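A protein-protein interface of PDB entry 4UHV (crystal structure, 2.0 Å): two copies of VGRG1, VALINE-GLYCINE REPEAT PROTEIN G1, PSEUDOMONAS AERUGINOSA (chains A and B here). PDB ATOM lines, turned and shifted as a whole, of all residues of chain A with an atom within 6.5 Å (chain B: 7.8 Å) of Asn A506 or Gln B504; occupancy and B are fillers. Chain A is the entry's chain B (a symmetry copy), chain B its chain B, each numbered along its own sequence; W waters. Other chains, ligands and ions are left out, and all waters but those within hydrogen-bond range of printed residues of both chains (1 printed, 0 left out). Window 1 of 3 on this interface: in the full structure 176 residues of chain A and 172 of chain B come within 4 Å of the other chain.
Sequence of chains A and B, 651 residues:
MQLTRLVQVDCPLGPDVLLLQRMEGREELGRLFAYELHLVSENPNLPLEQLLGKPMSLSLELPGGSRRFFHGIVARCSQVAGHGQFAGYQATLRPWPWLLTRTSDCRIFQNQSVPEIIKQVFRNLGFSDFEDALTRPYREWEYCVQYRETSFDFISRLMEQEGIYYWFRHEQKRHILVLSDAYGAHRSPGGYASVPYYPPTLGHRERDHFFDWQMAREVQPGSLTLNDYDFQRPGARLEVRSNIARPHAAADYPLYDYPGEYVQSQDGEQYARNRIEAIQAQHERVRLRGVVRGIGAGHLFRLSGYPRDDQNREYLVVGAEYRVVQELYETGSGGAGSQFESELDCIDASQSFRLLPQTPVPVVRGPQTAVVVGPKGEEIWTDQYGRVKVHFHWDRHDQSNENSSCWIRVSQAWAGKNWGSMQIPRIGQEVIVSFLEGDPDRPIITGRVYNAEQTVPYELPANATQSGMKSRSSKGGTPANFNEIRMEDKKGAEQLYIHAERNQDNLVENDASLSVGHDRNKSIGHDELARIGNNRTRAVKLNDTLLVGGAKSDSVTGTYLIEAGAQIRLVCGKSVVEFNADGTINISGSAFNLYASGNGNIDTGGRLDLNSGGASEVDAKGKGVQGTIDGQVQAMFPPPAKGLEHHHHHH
The side-chain carboxylate (OD2) of Asp A505 is in hydrogen-bond range of the side-chain amide nitrogen (NE2) of Gln B495, 3.0 Å away.
The backbone carbonyl oxygen of Leu B496 sits at hydrogen-bond distance from the backbone NH of Asp A505, 3.1 Å away.
O of Ile B498 lies within hydrogen-bond range of ND2 of Asn A506, at 3.0 Å.
The backbone NH (N) of Leu A507 lies within hydrogen-bond range of the backbone carbonyl oxygen (O) of Ile B498 (2.8 Å).
The backbone NH of Ala B500 sits at hydrogen-bond distance from the backbone carbonyl oxygen of Leu A507, at 2.7 Å.
The backbone NH (N) of Asn A510 sits at hydrogen-bond distance from the backbone carbonyl oxygen (O) of Arg B502, 2.6 Å away.
The side-chain amide nitrogen (ND2) of Asn A510 sits close to the side-chain amide oxygen (OD1) of Asn B503.
The backbone NH (N) of Asp A511 is in hydrogen-bond range of the side-chain amide oxygen (OD1) of Asn B503, 2.7 Å away.
OE1 of Gln B504 sits at hydrogen-bond distance from ND2 of Asn A506 (3.0 Å).
O of Asp A511 lies within hydrogen-bond range of N of Gln B504 (2.8 Å).
The backbone carbonyl oxygen (O) of Gln B504 is in hydrogen-bond range of the backbone NH (N) of Ser A513.
OG of Ser A513 sits at hydrogen-bond distance from OD1 of Asp B505 (3.1 Å).
The backbone carbonyl oxygen (O) of Ser A513 lies close to the backbone carbonyl oxygen (O) of Asn B506, 3.5 Å away.
The backbone carbonyl oxygen (O) of Glu B484 is in hydrogen-bond range of the backbone NH (N) of His B499 (2.6 Å).
Among the printed residues, pairs that only touch across the chains: Ala A512 with Gln B504, Val A508 with Gln B504, Gln A504 with Leu B496, Leu A507 with His B499, Val A508 with Arg B502, Val A508 with Ala B500, Leu A514 with Asn B506, Asp A511 with Arg B502 and Asp A505 with Ile B498.
Of the printed residues of chain B, Asp A505 touches Gln B495, Leu B496 and Ile B498.
Asn A506 touches two residues of chain B.
Tyr B497 touches none of the printed residues of chain A.
Printed residues of chain A within 4 Å of Ala B500: Leu A507 and Val A508.
Gln B504 touches just these residues of chain A: Asn A506, Val A508, Asp A511, Ala A512 and Ser A513.
Of the printed residues of chain A, Asp B505 touches Ser A513 (3.1 Å).
Asn B521 touches none of the printed residues of chain A.
The nearest residue of chain B that does not touch Asn A506 is His B499 (4.6 Å).
The nearest printed residue of chain A that does not touch Asn B506 is Ala A512 (6.2 Å).
Of the 10 printed residues of chain A, 10 touch a printed residue of chain B.
Of the 17 printed residues of chain B, 10 touch a printed residue of chain A.
Printed residues of chain B that touch a printed residue of chain A: Gln B495, Leu B496, Ile B498, His B499, Ala B500, Arg B502, Asn B503, Gln B504, Asp B505 and Asn B506.
Asn A506 touches Gln B504, but with the chains exchanged Gln A504 does not touch Asn B506 (8.6 Å).
Water W1 lies within hydrogen-bond range of the backbone carbonyl oxygen of Ile B498, the backbone NH of His B499 and the backbone carbonyl oxygen of Asp A505.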
ATOM      1  N   GLN A 504      25.395 -31.459  19.746  1.00  0.00           N
ATOM      2  CA  GLN A 504      25.550 -30.612  18.547  1.00  0.00           C
ATOM      3  C   GLN A 504      26.036 -29.247  18.974  1.00  0.00           C
ATOM      4  O   GLN A 504      25.498 -28.683  19.942  1.00  0.00           O
ATOM      5  CB  GLN A 504      24.217 -30.514  17.740  1.00  0.00           C
ATOM      6  CG  GLN A 504      24.356 -29.930  16.363  1.00  0.00           C
ATOM      7  CD  GLN A 504      23.060 -29.654  15.608  1.00  0.00           C
ATOM      8  OE1 GLN A 504      22.150 -30.463  15.588  1.00  0.00           O
ATOM      9  NE2 GLN A 504      23.039 -28.549  14.870  1.00  0.00           N
ATOM     10  N   ASP A 505      27.041 -28.699  18.254  1.00  0.00           N
ATOM     11  CA  ASP A 505      27.706 -27.460  18.698  1.00  0.00           C
ATOM     12  C   ASP A 505      27.973 -26.397  17.636  1.00  0.00           C
ATOM     13  O   ASP A 505      29.152 -26.103  17.292  1.00  0.00           O
ATOM     14  CB  ASP A 505      28.975 -27.842  19.476  1.00  0.00           C
ATOM     15  CG  ASP A 505      28.668 -28.778  20.657  1.00  0.00           C
ATOM     16  OD1 ASP A 505      28.192 -28.294  21.729  1.00  0.00           O
ATOM     17  OD2 ASP A 505      28.892 -30.023  20.520  1.00  0.00           O
ATOM     18  N   ASN A 506      26.906 -25.741  17.132  1.00  0.00           N
ATOM     19  CA  ASN A 506      26.988 -24.889  15.912  1.00  0.00           C
ATOM     20  C   ASN A 506      27.661 -23.577  16.227  1.00  0.00           C
ATOM     21  O   ASN A 506      27.375 -22.955  17.263  1.00  0.00           O
ATOM     22  CB  ASN A 506      25.560 -24.775  15.292  1.00  0.00           C
ATOM     23  CG  ASN A 506      25.452 -23.971  13.986  1.00  0.00           C
ATOM     24  OD1 ASN A 506      24.349 -23.721  13.590  1.00  0.00           O
ATOM     25  ND2 ASN A 506      26.521 -23.642  13.301  1.00  0.00           N
ATOM     26  N   LEU A 507      28.647 -23.167  15.432  1.00  0.00           N
ATOM     27  CA  LEU A 507      29.317 -21.901  15.648  1.00  0.00           C
ATOM     28  C   LEU A 507      29.314 -21.063  14.427  1.00  0.00           C
ATOM     29  O   LEU A 507      29.891 -21.476  13.378  1.00  0.00           O
ATOM     30  CB  LEU A 507      30.781 -22.123  15.998  1.00  0.00           C
ATOM     31  CG  LEU A 507      31.451 -20.868  16.499  1.00  0.00           C
ATOM     32  CD1 LEU A 507      31.141 -20.684  17.979  1.00  0.00           C
ATOM     33  CD2 LEU A 507      32.908 -21.018  16.308  1.00  0.00           C
ATOM     34  N   VAL A 508      28.739 -19.880  14.570  1.00  0.00           N
ATOM     35  CA  VAL A 508      28.628 -18.895  13.524  1.00  0.00           C
ATOM     36  C   VAL A 508      29.438 -17.630  13.867  1.00  0.00           C
ATOM     37  O   VAL A 508      29.193 -17.000  14.925  1.00  0.00           O
ATOM     38  CB  VAL A 508      27.148 -18.594  13.315  1.00  0.00           C
ATOM     39  CG1 VAL A 508      26.970 -17.360  12.464  1.00  0.00           C
ATOM     40  CG2 VAL A 508      26.471 -19.801  12.672  1.00  0.00           C
ATOM     41  N   ASN A 510      30.163 -14.480  12.246  1.00  0.00           N
ATOM     42  CA  ASN A 510      29.393 -13.220  12.182  1.00  0.00           C
ATOM     43  C   ASN A 510      27.866 -13.377  12.429  1.00  0.00           C
ATOM     44  O   ASN A 510      27.461 -13.452  13.564  1.00  0.00           O
ATOM     45  CB  ASN A 510      29.716 -12.455  10.904  1.00  0.00           C
ATOM     46  CG  ASN A 510      29.168 -11.035  10.916  1.00  0.00           C
ATOM     47  OD1 ASN A 510      29.547 -10.213  11.770  1.00  0.00           O
ATOM     48  ND2 ASN A 510      28.310 -10.730   9.973  1.00  0.00           N
ATOM     49  N   ASP A 511      27.021 -13.401  11.403  1.00  0.00           N
ATOM     50  CA  ASP A 511      25.580 -13.427  11.545  1.00  0.00           C
ATOM     51  C   ASP A 511      24.914 -14.690  11.079  1.00  0.00           C
ATOM     52  O   ASP A 511      25.444 -15.394  10.224  1.00  0.00           O
ATOM     53  CB  ASP A 511      24.973 -12.399  10.626  1.00  0.00           C
ATOM     54  CG  ASP A 511      24.969 -11.050  11.206  1.00  0.00           C
ATOM     55  OD1 ASP A 511      25.398 -10.913  12.367  1.00  0.00           O
ATOM     56  OD2 ASP A 511      24.555 -10.128  10.464  1.00  0.00           O
ATOM     57  N   ALA A 512      23.685 -14.879  11.541  1.00  0.00           N
ATOM     58  CA  ALA A 512      22.878 -16.050  11.200  1.00  0.00           C
ATOM     59  C   ALA A 512      21.477 -15.569  10.930  1.00  0.00           C
ATOM     60  O   ALA A 512      21.055 -14.590  11.524  1.00  0.00           O
ATOM     61  CB  ALA A 512      22.892 -17.054  12.335  1.00  0.00           C
ATOM     62  N   SER A 513      20.714 -16.273  10.091  1.00  0.00           N
ATOM     63  CA  SER A 513      19.402 -15.755   9.667  1.00  0.00           C
ATOM     64  C   SER A 513      18.388 -16.828   9.436  1.00  0.00           C
ATOM     65  O   SER A 513      18.053 -17.092   8.286  1.00  0.00           O
ATOM     66  CB  SER A 513      19.535 -14.964   8.343  1.00  0.00           C
ATOM     67  OG  SER A 513      20.452 -13.913   8.437  1.00  0.00           O
ATOM     68  N   LEU A 514      17.829 -17.431  10.493  1.00  0.00           N
ATOM     69  CA  LEU A 514      16.833 -18.460  10.271  1.00  0.00           C
ATOM     70  C   LEU A 514      15.440 -17.921   9.766  1.00  0.00           C
ATOM     71  O   LEU A 514      14.728 -17.187  10.439  1.00  0.00           O
ATOM     72  CB  LEU A 514      16.704 -19.364  11.506  1.00  0.00           C
ATOM     73  CG  LEU A 514      15.526 -20.335  11.591  1.00  0.00           C
ATOM     74  CD1 LEU A 514      15.453 -21.299  10.417  1.00  0.00           C
ATOM     75  CD2 LEU A 514      15.523 -21.120  12.901  1.00  0.00           C
ATOM     76  N   ASN B 483      34.772 -23.078   6.993  1.00  0.00           N
ATOM     77  CA  ASN B 483      33.454 -23.595   7.264  1.00  0.00           C
ATOM     78  C   ASN B 483      33.576 -25.111   7.435  1.00  0.00           C
ATOM     79  O   ASN B 483      34.241 -25.791   6.633  1.00  0.00           O
ATOM     80  CB  ASN B 483      32.523 -23.273   6.095  1.00  0.00           C
ATOM     81  CG  ASN B 483      32.525 -21.801   5.713  1.00  0.00           C
ATOM     82  OD1 ASN B 483      32.198 -20.925   6.544  1.00  0.00           O
ATOM     83  ND2 ASN B 483      32.852 -21.509   4.441  1.00  0.00           N
ATOM     84  N   GLU B 484      32.995 -25.689   8.469  1.00  0.00           N
ATOM     85  CA  GLU B 484      33.137 -27.176   8.616  1.00  0.00           C
ATOM     86  C   GLU B 484      31.892 -27.843   9.155  1.00  0.00           C
ATOM     87  O   GLU B 484      31.166 -27.239   9.937  1.00  0.00           O
ATOM     88  CB  GLU B 484      34.335 -27.513   9.497  1.00  0.00           C
ATOM     89  CG  GLU B 484      34.277 -28.865  10.170  1.00  0.00           C
ATOM     90  CD  GLU B 484      35.520 -29.231  10.904  1.00  0.00           C
ATOM     91  OE1 GLU B 484      36.324 -28.365  11.231  1.00  0.00           O
ATOM     92  OE2 GLU B 484      35.725 -30.418  11.182  1.00  0.00           O
ATOM     93  N   GLN B 495      29.291 -36.361  18.530  1.00  0.00           N
ATOM     94  CA  GLN B 495      29.014 -34.952  18.345  1.00  0.00           C
ATOM     95  C   GLN B 495      28.769 -34.625  16.889  1.00  0.00           C
ATOM     96  O   GLN B 495      29.282 -35.299  15.995  1.00  0.00           O
ATOM     97  CB  GLN B 495      30.216 -34.170  18.897  1.00  0.00           C
ATOM     98  CG  GLN B 495      30.102 -32.668  18.938  1.00  0.00           C
ATOM     99  CD  GLN B 495      31.397 -32.039  19.393  1.00  0.00           C
ATOM    100  OE1 GLN B 495      32.328 -32.730  19.906  1.00  0.00           O
ATOM    101  NE2 GLN B 495      31.483 -30.745  19.242  1.00  0.00           N
ATOM    102  N   LEU B 496      27.974 -33.594  16.637  1.00  0.00           N
ATOM    103  CA  LEU B 496      27.869 -33.069  15.302  1.00  0.00           C
ATOM    104  C   LEU B 496      28.254 -31.594  15.381  1.00  0.00           C
ATOM    105  O   LEU B 496      27.591 -30.778  16.023  1.00  0.00           O
ATOM    106  CB  LEU B 496      26.480 -33.313  14.705  1.00  0.00           C
ATOM    107  CG  LEU B 496      26.304 -32.986  13.218  1.00  0.00           C
ATOM    108  CD1 LEU B 496      27.307 -33.771  12.342  1.00  0.00           C
ATOM    109  CD2 LEU B 496      24.865 -33.268  12.801  1.00  0.00           C
ATOM    110  N   TYR B 497      29.345 -31.252  14.717  1.00  0.00           N
ATOM    111  CA  TYR B 497      29.827 -29.918  14.792  1.00  0.00           C
ATOM    112  C   TYR B 497      29.753 -29.192  13.410  1.00  0.00           C
ATOM    113  O   TYR B 497      30.380 -29.626  12.422  1.00  0.00           O
ATOM    114  CB  TYR B 497      31.191 -30.040  15.459  1.00  0.00           C
ATOM    115  CG  TYR B 497      32.147 -28.937  15.330  1.00  0.00           C
ATOM    116  CD1 TYR B 497      32.526 -28.459  14.099  1.00  0.00           C
ATOM    117  CD2 TYR B 497      32.730 -28.361  16.461  1.00  0.00           C
ATOM    118  CE1 TYR B 497      33.445 -27.459  13.983  1.00  0.00           C
ATOM    119  CE2 TYR B 497      33.667 -27.380  16.331  1.00  0.00           C
ATOM    120  CZ  TYR B 497      34.014 -26.939  15.076  1.00  0.00           C
ATOM    121  OH  TYR B 497      34.935 -25.952  14.910  1.00  0.00           O
ATOM    122  N   ILE B 498      28.940 -28.128  13.358  1.00  0.00           N
ATOM    123  CA  ILE B 498      28.841 -27.171  12.261  1.00  0.00           C
ATOM    124  C   ILE B 498      29.516 -25.795  12.533  1.00  0.00           C
ATOM    125  O   ILE B 498      29.144 -25.065  13.492  1.00  0.00           O
ATOM    126  CB  ILE B 498      27.355 -26.868  11.913  1.00  0.00           C
ATOM    127  CG1 ILE B 498      26.563 -28.164  11.709  1.00  0.00           C
ATOM    128  CG2 ILE B 498      27.268 -25.950  10.678  1.00  0.00           C
ATOM    129  CD1 ILE B 498      25.212 -27.991  11.075  1.00  0.00           C
ATOM    130  N   HIS B 499      30.430 -25.382  11.665  1.00  0.00           N
ATOM    131  CA  HIS B 499      31.213 -24.165  11.875  1.00  0.00           C
ATOM    132  C   HIS B 499      31.089 -23.272  10.680  1.00  0.00           C
ATOM    133  O   HIS B 499      31.564 -23.625   9.591  1.00  0.00           O
ATOM    134  CB  HIS B 499      32.672 -24.543  12.068  1.00  0.00           C
ATOM    135  CG  HIS B 499      33.564 -23.380  12.360  1.00  0.00           C
ATOM    136  ND1 HIS B 499      34.058 -22.543  11.371  1.00  0.00           N
ATOM    137  CD2 HIS B 499      34.029 -22.901  13.530  1.00  0.00           C
ATOM    138  CE1 HIS B 499      34.803 -21.608  11.931  1.00  0.00           C
ATOM    139  NE2 HIS B 499      34.831 -21.830  13.235  1.00  0.00           N
ATOM    140  N   ALA B 500      30.433 -22.113  10.848  1.00  0.00           N
ATOM    141  CA  ALA B 500      30.328 -21.151   9.774  1.00  0.00           C
ATOM    142  C   ALA B 500      31.357 -20.047  10.068  1.00  0.00           C
ATOM    143  O   ALA B 500      31.269 -19.328  11.111  1.00  0.00           O
ATOM    144  CB  ALA B 500      28.893 -20.595   9.681  1.00  0.00           C
ATOM    145  N   GLU B 501      32.324 -19.956   9.149  1.00  0.00           N
ATOM    146  CA  GLU B 501      33.455 -19.082   9.222  1.00  0.00           C
ATOM    147  C   GLU B 501      33.044 -17.608   9.233  1.00  0.00           C
ATOM    148  O   GLU B 501      33.774 -16.781   9.737  1.00  0.00           O
ATOM    149  CB  GLU B 501      34.369 -19.335   8.019  1.00  0.00           C
ATOM    150  CG  GLU B 501      35.443 -18.288   7.793  1.00  0.00           C
ATOM    151  CD  GLU B 501      36.305 -18.102   9.028  1.00  0.00           C
ATOM    152  OE1 GLU B 501      36.439 -19.049   9.780  1.00  0.00           O
ATOM    153  OE2 GLU B 501      36.850 -17.020   9.257  1.00  0.00           O
ATOM    154  N   ARG B 502      31.916 -17.281   8.629  1.00  0.00           N
ATOM    155  CA  ARG B 502      31.321 -15.988   8.813  1.00  0.00           C
ATOM    156  C   ARG B 502      29.843 -16.094   9.101  1.00  0.00           C
ATOM    157  O   ARG B 502      29.466 -16.045  10.252  1.00  0.00           O
ATOM    158  CB  ARG B 502      31.547 -15.108   7.633  1.00  0.00           C
ATOM    159  CG  ARG B 502      32.748 -14.248   7.760  1.00  0.00           C
ATOM    160  CD  ARG B 502      32.548 -13.012   6.925  1.00  0.00           C
ATOM    161  NE  ARG B 502      32.874 -11.817   7.680  1.00  0.00           N
ATOM    162  CZ  ARG B 502      32.297 -10.643   7.452  1.00  0.00           C
ATOM    163  NH1 ARG B 502      31.392 -10.547   6.495  1.00  0.00           N
ATOM    164  NH2 ARG B 502      32.615  -9.565   8.167  1.00  0.00           N
ATOM    165  N   ASN B 503      29.022 -16.215   8.062  1.00  0.00           N
ATOM    166  CA  ASN B 503      27.562 -16.057   8.155  1.00  0.00           C
ATOM    167  C   ASN B 503      26.794 -17.309   7.774  1.00  0.00           C
ATOM    168  O   ASN B 503      27.305 -18.143   7.004  1.00  0.00           O
ATOM    169  CB  ASN B 503      27.135 -14.910   7.262  1.00  0.00           C
ATOM    170  CG  ASN B 503      27.377 -13.569   7.891  1.00  0.00           C
ATOM    171  OD1 ASN B 503      27.984 -13.474   8.934  1.00  0.00           O
ATOM    172  ND2 ASN B 503      26.927 -12.539   7.254  1.00  0.00           N
ATOM    173  N   GLN B 504      25.645 -17.530   8.414  1.00  0.00           N
ATOM    174  CA  GLN B 504      24.828 -18.733   8.158  1.00  0.00           C
ATOM    175  C   GLN B 504      23.405 -18.306   7.882  1.00  0.00           C
ATOM    176  O   GLN B 504      22.869 -17.461   8.619  1.00  0.00           O
ATOM    177  CB  GLN B 504      24.899 -19.737   9.352  1.00  0.00           C
ATOM    178  CG  GLN B 504      24.353 -21.104   9.057  1.00  0.00           C
ATOM    179  CD  GLN B 504      24.241 -22.060  10.240  1.00  0.00           C
ATOM    180  OE1 GLN B 504      25.142 -22.177  11.051  1.00  0.00           O
ATOM    181  NE2 GLN B 504      23.172 -22.847  10.255  1.00  0.00           N
ATOM    182  N   ASP B 505      22.780 -18.891   6.837  1.00  0.00           N
ATOM    183  CA  ASP B 505      21.462 -18.415   6.376  1.00  0.00           C
ATOM    184  C   ASP B 505      20.414 -19.477   6.052  1.00  0.00           C
ATOM    185  O   ASP B 505      20.010 -19.651   4.869  1.00  0.00           O
ATOM    186  CB  ASP B 505      21.681 -17.435   5.212  1.00  0.00           C
ATOM    187  CG  ASP B 505      22.602 -16.268   5.605  1.00  0.00           C
ATOM    188  OD1 ASP B 505      22.135 -15.308   6.289  1.00  0.00           O
ATOM    189  OD2 ASP B 505      23.821 -16.307   5.241  1.00  0.00           O
ATOM    190  N   ASN B 506      19.893 -20.170   7.088  1.00  0.00           N
ATOM    191  CA  ASN B 506      19.080 -21.404   6.900  1.00  0.00           C
ATOM    192  C   ASN B 506      17.694 -21.057   6.419  1.00  0.00           C
ATOM    193  O   ASN B 506      17.070 -20.110   6.924  1.00  0.00           O
ATOM    194  CB  ASN B 506      19.140 -22.239   8.218  1.00  0.00           C
ATOM    195  CG  ASN B 506      18.397 -23.585   8.200  1.00  0.00           C
ATOM    196  OD1 ASN B 506      18.279 -24.156   9.246  1.00  0.00           O
ATOM    197  ND2 ASN B 506      17.980 -24.115   7.074  1.00  0.00           N
ATOM    198  N   LEU B 507      17.210 -21.713   5.366  1.00  0.00           N
ATOM    199  CA  LEU B 507      15.874 -21.462   4.867  1.00  0.00           C
ATOM    200  C   LEU B 507      15.083 -22.711   4.762  1.00  0.00           C
ATOM    201  O   LEU B 507      15.468 -23.637   3.990  1.00  0.00           O
ATOM    202  CB  LEU B 507      15.927 -20.883   3.461  1.00  0.00           C
ATOM    203  CG  LEU B 507      14.591 -20.349   3.005  1.00  0.00           C
ATOM    204  CD1 LEU B 507      14.390 -18.945   3.560  1.00  0.00           C
ATOM    205  CD2 LEU B 507      14.593 -20.310   1.529  1.00  0.00           C
ATOM    206  N   ASN B 521      22.021 -24.416  25.128  1.00  0.00           N
ATOM    207  CA  ASN B 521      22.572 -23.142  25.563  1.00  0.00           C
ATOM    208  C   ASN B 521      22.775 -22.341  24.289  1.00  0.00           C
ATOM    209  O   ASN B 521      23.667 -22.687  23.526  1.00  0.00           O
ATOM    210  CB  ASN B 521      23.906 -23.399  26.351  1.00  0.00           C
ATOM    211  CG  ASN B 521      24.728 -22.132  26.646  1.00  0.00           C
ATOM    212  OD1 ASN B 521      24.439 -21.348  27.556  1.00  0.00           O
ATOM    213  ND2 ASN B 521      25.814 -21.982  25.929  1.00  0.00           N
ATOM    214  N   SER B 523      23.842 -18.633  22.777  1.00  0.00           N
ATOM    215  CA  SER B 523      24.485 -17.390  23.164  1.00  0.00           C
ATOM    216  C   SER B 523      24.794 -16.616  21.916  1.00  0.00           C
ATOM    217  O   SER B 523      25.600 -17.057  21.116  1.00  0.00           O
ATOM    218  CB  SER B 523      25.801 -17.664  23.966  1.00  0.00           C
ATOM    219  OG  SER B 523      25.471 -18.015  25.309  1.00  0.00           O
HETATM  220  O   HOH W   1      31.225 -25.462  14.816  1.00  0.00           O
